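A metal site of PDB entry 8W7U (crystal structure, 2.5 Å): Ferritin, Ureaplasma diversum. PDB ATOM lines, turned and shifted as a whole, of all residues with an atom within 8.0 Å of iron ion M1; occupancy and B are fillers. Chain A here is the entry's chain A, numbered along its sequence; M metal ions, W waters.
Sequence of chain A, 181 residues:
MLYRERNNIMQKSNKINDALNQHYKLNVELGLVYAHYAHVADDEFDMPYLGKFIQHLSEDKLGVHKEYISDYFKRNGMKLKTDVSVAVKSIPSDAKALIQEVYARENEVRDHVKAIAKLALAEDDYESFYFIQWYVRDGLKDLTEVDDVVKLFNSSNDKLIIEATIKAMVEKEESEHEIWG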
ATOM      1  N   ASN A  27      -9.224  22.344  -7.490  1.00  0.00           N
ATOM      2  CA  ASN A  27      -9.749  21.060  -7.863  1.00  0.00           C
ATOM      3  C   ASN A  27      -8.677  20.022  -8.112  1.00  0.00           C
ATOM      4  O   ASN A  27      -8.837  18.888  -7.764  1.00  0.00           O
ATOM      5  CB  ASN A  27     -10.730  21.220  -9.014  1.00  0.00           C
ATOM      6  CG  ASN A  27     -12.107  21.518  -8.559  1.00  0.00           C
ATOM      7  OD1 ASN A  27     -12.745  20.666  -8.002  1.00  0.00           O
ATOM      8  ND2 ASN A  27     -12.565  22.723  -8.790  1.00  0.00           N
ATOM      9  N   HIS A  56     -13.371   8.171  -5.655  1.00  0.00           N
ATOM     10  CA  HIS A  56     -14.350   8.611  -6.624  1.00  0.00           C
ATOM     11  C   HIS A  56     -14.442  10.119  -6.617  1.00  0.00           C
ATOM     12  O   HIS A  56     -14.558  10.743  -7.643  1.00  0.00           O
ATOM     13  CB  HIS A  56     -15.692   7.927  -6.417  1.00  0.00           C
ATOM     14  CG  HIS A  56     -16.805   8.519  -7.220  1.00  0.00           C
ATOM     15  ND1 HIS A  56     -16.927   8.331  -8.572  1.00  0.00           N
ATOM     16  CD2 HIS A  56     -17.849   9.302  -6.847  1.00  0.00           C
ATOM     17  CE1 HIS A  56     -17.997   8.970  -9.004  1.00  0.00           C
ATOM     18  NE2 HIS A  56     -18.568   9.570  -7.984  1.00  0.00           N
ATOM     19  N   LEU A  57     -14.309  10.713  -5.456  1.00  0.00           N
ATOM     20  CA  LEU A  57     -14.274  12.142  -5.352  1.00  0.00           C
ATOM     21  C   LEU A  57     -12.992  12.748  -5.877  1.00  0.00           C
ATOM     22  O   LEU A  57     -13.006  13.823  -6.383  1.00  0.00           O
ATOM     23  CB  LEU A  57     -14.476  12.543  -3.907  1.00  0.00           C
ATOM     24  CG  LEU A  57     -15.696  12.145  -3.107  1.00  0.00           C
ATOM     25  CD1 LEU A  57     -15.637  12.881  -1.795  1.00  0.00           C
ATOM     26  CD2 LEU A  57     -16.997  12.433  -3.837  1.00  0.00           C
ATOM     27  N   GLU A  59     -11.367  11.620  -8.399  1.00  0.00           N
ATOM     28  CA  GLU A  59     -11.542  11.577  -9.812  1.00  0.00           C
ATOM     29  C   GLU A  59     -12.541  12.578 -10.346  1.00  0.00           C
ATOM     30  O   GLU A  59     -12.426  12.958 -11.472  1.00  0.00           O
ATOM     31  CB  GLU A  59     -11.874  10.158 -10.181  1.00  0.00           C
ATOM     32  CG  GLU A  59     -10.711   9.200 -10.080  1.00  0.00           C
ATOM     33  CD  GLU A  59     -11.161   7.765  -9.961  1.00  0.00           C
ATOM     34  OE1 GLU A  59     -10.322   6.902  -9.676  1.00  0.00           O
ATOM     35  OE2 GLU A  59     -12.355   7.490 -10.137  1.00  0.00           O
ATOM     36  N   ASP A  60     -13.455  13.018  -9.539  1.00  0.00           N
ATOM     37  CA  ASP A  60     -14.372  14.019  -9.917  1.00  0.00           C
ATOM     38  C   ASP A  60     -13.653  15.360  -9.978  1.00  0.00           C
ATOM     39  O   ASP A  60     -13.788  16.084 -10.914  1.00  0.00           O
ATOM     40  CB  ASP A  60     -15.381  13.967  -8.809  1.00  0.00           C
ATOM     41  CG  ASP A  60     -16.666  14.482  -9.169  1.00  0.00           C
ATOM     42  OD1 ASP A  60     -17.204  15.221  -8.340  1.00  0.00           O
ATOM     43  OD2 ASP A  60     -17.121  14.145 -10.270  1.00  0.00           O
ATOM     44  N   LYS A  61     -12.864  15.647  -8.988  1.00  0.00           N
ATOM     45  CA  LYS A  61     -12.105  16.866  -8.916  1.00  0.00           C
ATOM     46  C   LYS A  61     -11.032  16.963  -9.989  1.00  0.00           C
ATOM     47  O   LYS A  61     -10.855  18.002 -10.567  1.00  0.00           O
ATOM     48  CB  LYS A  61     -11.522  17.047  -7.520  1.00  0.00           C
ATOM     49  CG  LYS A  61     -12.441  16.964  -6.325  1.00  0.00           C
ATOM     50  CD  LYS A  61     -13.627  17.901  -6.425  1.00  0.00           C
ATOM     51  CE  LYS A  61     -14.387  17.895  -5.126  1.00  0.00           C
ATOM     52  NZ  LYS A  61     -15.584  18.777  -5.178  1.00  0.00           N
ATOM     53  N   VAL A  64     -14.056  16.053 -14.279  1.00  0.00           N
ATOM     54  CA  VAL A  64     -15.035  17.023 -14.662  1.00  0.00           C
ATOM     55  C   VAL A  64     -14.917  18.422 -14.085  1.00  0.00           C
ATOM     56  O   VAL A  64     -15.108  19.369 -14.798  1.00  0.00           O
ATOM     57  CB  VAL A  64     -16.477  16.496 -14.525  1.00  0.00           C
ATOM     58  CG1 VAL A  64     -16.731  15.364 -15.495  1.00  0.00           C
ATOM     59  CG2 VAL A  64     -16.821  16.117 -13.095  1.00  0.00           C
ATOM     60  N   HIS A  65     -14.568  18.540 -12.828  1.00  0.00           N
ATOM     61  CA  HIS A  65     -14.440  19.820 -12.195  1.00  0.00           C
ATOM     62  C   HIS A  65     -13.366  20.649 -12.845  1.00  0.00           C
ATOM     63  O   HIS A  65     -13.512  21.838 -12.964  1.00  0.00           O
ATOM     64  CB  HIS A  65     -14.155  19.620 -10.739  1.00  0.00           C
ATOM     65  CG  HIS A  65     -15.342  19.305  -9.892  1.00  0.00           C
ATOM     66  ND1 HIS A  65     -15.908  20.221  -9.042  1.00  0.00           N
ATOM     67  CD2 HIS A  65     -16.035  18.162  -9.723  1.00  0.00           C
ATOM     68  CE1 HIS A  65     -16.904  19.659  -8.400  1.00  0.00           C
ATOM     69  NE2 HIS A  65     -17.014  18.409  -8.800  1.00  0.00           N
ATOM     70  N   GLU A 106     -14.995  20.571   1.228  1.00  0.00           N
ATOM     71  CA  GLU A 106     -16.152  20.754   0.381  1.00  0.00           C
ATOM     72  C   GLU A 106     -16.946  21.978   0.739  1.00  0.00           C
ATOM     73  O   GLU A 106     -17.444  22.633  -0.135  1.00  0.00           O
ATOM     74  CB  GLU A 106     -17.048  19.510   0.399  1.00  0.00           C
ATOM     75  CG  GLU A 106     -16.392  18.227  -0.021  1.00  0.00           C
ATOM     76  CD  GLU A 106     -15.930  18.237  -1.456  1.00  0.00           C
ATOM     77  OE1 GLU A 106     -16.639  18.760  -2.323  1.00  0.00           O
ATOM     78  OE2 GLU A 106     -14.854  17.697  -1.712  1.00  0.00           O
ATOM     79  N   VAL A 109     -15.350  24.983  -0.734  1.00  0.00           N
ATOM     80  CA  VAL A 109     -15.609  25.081  -2.131  1.00  0.00           C
ATOM     81  C   VAL A 109     -16.875  25.841  -2.370  1.00  0.00           C
ATOM     82  O   VAL A 109     -16.945  26.665  -3.252  1.00  0.00           O
ATOM     83  CB  VAL A 109     -15.655  23.672  -2.760  1.00  0.00           C
ATOM     84  CG1 VAL A 109     -16.304  23.663  -4.133  1.00  0.00           C
ATOM     85  CG2 VAL A 109     -14.292  23.031  -2.770  1.00  0.00           C
ATOM     86  N   TRP A 134     -23.289  25.069 -12.412  1.00  0.00           N
ATOM     87  CA  TRP A 134     -22.987  23.666 -12.249  1.00  0.00           C
ATOM     88  C   TRP A 134     -22.270  23.483 -10.960  1.00  0.00           C
ATOM     89  O   TRP A 134     -22.562  22.588 -10.220  1.00  0.00           O
ATOM     90  CB  TRP A 134     -22.133  23.191 -13.436  1.00  0.00           C
ATOM     91  CG  TRP A 134     -21.868  21.727 -13.516  1.00  0.00           C
ATOM     92  CD1 TRP A 134     -22.571  20.816 -14.219  1.00  0.00           C
ATOM     93  CD2 TRP A 134     -20.810  21.010 -12.882  1.00  0.00           C
ATOM     94  NE1 TRP A 134     -22.036  19.580 -14.069  1.00  0.00           N
ATOM     95  CE2 TRP A 134     -20.957  19.668 -13.239  1.00  0.00           C
ATOM     96  CE3 TRP A 134     -19.771  21.361 -12.035  1.00  0.00           C
ATOM     97  CZ2 TRP A 134     -20.098  18.677 -12.782  1.00  0.00           C
ATOM     98  CZ3 TRP A 134     -18.919  20.392 -11.581  1.00  0.00           C
ATOM     99  CH2 TRP A 134     -19.079  19.066 -11.959  1.00  0.00           C
ATOM    100  N   TYR A 135     -21.337  24.361 -10.703  1.00  0.00           N
ATOM    101  CA  TYR A 135     -20.572  24.325  -9.505  1.00  0.00           C
ATOM    102  C   TYR A 135     -21.309  24.768  -8.239  1.00  0.00           C
ATOM    103  O   TYR A 135     -20.949  24.357  -7.174  1.00  0.00           O
ATOM    104  CB  TYR A 135     -19.274  25.122  -9.756  1.00  0.00           C
ATOM    105  CG  TYR A 135     -18.390  24.630 -10.863  1.00  0.00           C
ATOM    106  CD1 TYR A 135     -18.635  24.970 -12.181  1.00  0.00           C
ATOM    107  CD2 TYR A 135     -17.292  23.847 -10.589  1.00  0.00           C
ATOM    108  CE1 TYR A 135     -17.824  24.514 -13.188  1.00  0.00           C
ATOM    109  CE2 TYR A 135     -16.478  23.392 -11.587  1.00  0.00           C
ATOM    110  CZ  TYR A 135     -16.747  23.736 -12.888  1.00  0.00           C
ATOM    111  OH  TYR A 135     -15.931  23.284 -13.876  1.00  0.00           O
ATOM    112  N   ARG A 137     -24.385  24.033  -7.827  1.00  0.00           N
ATOM    113  CA  ARG A 137     -25.140  22.840  -7.586  1.00  0.00           C
ATOM    114  C   ARG A 137     -24.329  21.678  -7.086  1.00  0.00           C
ATOM    115  O   ARG A 137     -24.717  21.038  -6.140  1.00  0.00           O
ATOM    116  CB  ARG A 137     -25.907  22.493  -8.846  1.00  0.00           C
ATOM    117  CG  ARG A 137     -26.811  21.293  -8.761  1.00  0.00           C
ATOM    118  CD  ARG A 137     -26.889  20.553 -10.088  1.00  0.00           C
ATOM    119  NE  ARG A 137     -25.620  20.427 -10.774  1.00  0.00           N
ATOM    120  CZ  ARG A 137     -24.693  19.511 -10.504  1.00  0.00           C
ATOM    121  NH1 ARG A 137     -24.867  18.645  -9.539  1.00  0.00           N
ATOM    122  NH2 ARG A 137     -23.583  19.497 -11.199  1.00  0.00           N
ATOM    123  N   ASP A 138     -23.199  21.416  -7.689  1.00  0.00           N
ATOM    124  CA  ASP A 138     -22.354  20.318  -7.288  1.00  0.00           C
ATOM    125  C   ASP A 138     -21.777  20.591  -5.932  1.00  0.00           C
ATOM    126  O   ASP A 138     -21.469  19.686  -5.232  1.00  0.00           O
ATOM    127  CB  ASP A 138     -21.277  19.992  -8.342  1.00  0.00           C
ATOM    128  CG  ASP A 138     -21.066  18.538  -8.535  1.00  0.00           C
ATOM    129  OD1 ASP A 138     -22.022  17.849  -8.881  1.00  0.00           O
ATOM    130  OD2 ASP A 138     -19.930  18.072  -8.367  1.00  0.00           O
ATOM    131  N   GLY A 139     -21.670  21.853  -5.545  1.00  0.00           N
ATOM    132  CA  GLY A 139     -21.209  22.210  -4.226  1.00  0.00           C
ATOM    133  C   GLY A 139     -22.041  21.666  -3.124  1.00  0.00           C
ATOM    134  O   GLY A 139     -21.532  21.114  -2.180  1.00  0.00           O
ATOM    135  N   LYS A 141     -24.380  19.214  -3.584  1.00  0.00           N
ATOM    136  CA  LYS A 141     -24.459  17.790  -3.792  1.00  0.00           C
ATOM    137  C   LYS A 141     -23.277  17.045  -3.286  1.00  0.00           C
ATOM    138  O   LYS A 141     -23.406  15.985  -2.739  1.00  0.00           O
ATOM    139  CB  LYS A 141     -24.633  17.506  -5.279  1.00  0.00           C
ATOM    140  CG  LYS A 141     -24.964  16.090  -5.671  1.00  0.00           C
ATOM    141  CD  LYS A 141     -24.009  15.648  -6.746  1.00  0.00           C
ATOM    142  CE  LYS A 141     -24.640  14.626  -7.660  1.00  0.00           C
ATOM    143  NZ  LYS A 141     -23.886  14.529  -8.935  1.00  0.00           N
ATOM    144  N   ASP A 142     -22.120  17.622  -3.445  1.00  0.00           N
ATOM    145  CA  ASP A 142     -20.936  16.981  -3.027  1.00  0.00           C
ATOM    146  C   ASP A 142     -20.834  17.018  -1.538  1.00  0.00           C
ATOM    147  O   ASP A 142     -20.390  16.069  -0.943  1.00  0.00           O
ATOM    148  CB  ASP A 142     -19.713  17.556  -3.751  1.00  0.00           C
ATOM    149  CG  ASP A 142     -19.578  17.078  -5.180  1.00  0.00           C
ATOM    150  OD1 ASP A 142     -20.390  16.256  -5.614  1.00  0.00           O
ATOM    151  OD2 ASP A 142     -18.648  17.527  -5.872  1.00  0.00           O
ATOM    152  N   LEU A 143     -21.312  18.087  -0.919  1.00  0.00           N
ATOM    153  CA  LEU A 143     -21.348  18.147   0.521  1.00  0.00           C
ATOM    154  C   LEU A 143     -22.329  17.190   1.109  1.00  0.00           C
ATOM    155  O   LEU A 143     -22.103  16.642   2.148  1.00  0.00           O
ATOM    156  CB  LEU A 143     -21.675  19.559   0.984  1.00  0.00           C
ATOM    157  CG  LEU A 143     -21.475  19.924   2.444  1.00  0.00           C
ATOM    158  CD1 LEU A 143     -20.085  20.451   2.664  1.00  0.00           C
ATOM    159  CD2 LEU A 143     -22.511  20.916   2.906  1.00  0.00           C
ATOM    160  N   GLU A 145     -23.241  14.314  -0.145  1.00  0.00           N
ATOM    161  CA  GLU A 145     -22.693  12.990  -0.192  1.00  0.00           C
ATOM    162  C   GLU A 145     -21.722  12.726   0.922  1.00  0.00           C
ATOM    163  O   GLU A 145     -21.760  11.693   1.520  1.00  0.00           O
ATOM    164  CB  GLU A 145     -22.062  12.714  -1.549  1.00  0.00           C
ATOM    165  CG  GLU A 145     -23.003  12.652  -2.726  1.00  0.00           C
ATOM    166  CD  GLU A 145     -22.270  12.218  -3.982  1.00  0.00           C
ATOM    167  OE1 GLU A 145     -22.941  12.003  -5.013  1.00  0.00           O
ATOM    168  OE2 GLU A 145     -21.024  12.082  -3.932  1.00  0.00           O
HETATM  169 FE    FE M   1     -18.558  16.960  -7.695  1.00  0.00          FE
HETATM  170 FE    FE M   2     -20.141  10.926  -8.073  1.00  0.00          FE
HETATM  171  O   HOH W   1     -19.576  15.525  -9.692  1.00  0.00           O
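The side-chain amide oxygen (OD1) of Asn 27 lies close to a ring nitrogen (ND1) of His 65 (3.4 Å). NZ of Lys 141 lies within salt-bridge range of OD1 of Asp 138, at 3.8 Å. NH1 of Arg 137 is in salt-bridge range of OD1 of Asp 138, 3.0 Å away. OD2 of Asp 142 sits close to NZ of Lys 61. O of His 65 lies within hydrogen-bond range of OH of Tyr 135 (3.0 Å).
The nearest printed residue that does not touch iron ion M1 is Lys 61 (4.3 Å).
Iron ion M1 is bound by OD2 of Asp 138 (1.9 Å), OD2 of Asp 142 (1.9 Å), OD1 of Asp 60 (2.3 Å) and NE2 of His 65 (2.4 Å). Iron ion M1 has four donor atoms within binding distance. Slightly farther from iron ion M1 lies water W1 (2.7 Å).
Water W1 lies within hydrogen-bond range of the side-chain carboxylate (OD2) of Asp 60 (2.9 Å) and the side-chain carboxylate (OD1) of Asp 138 (3.5 Å).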
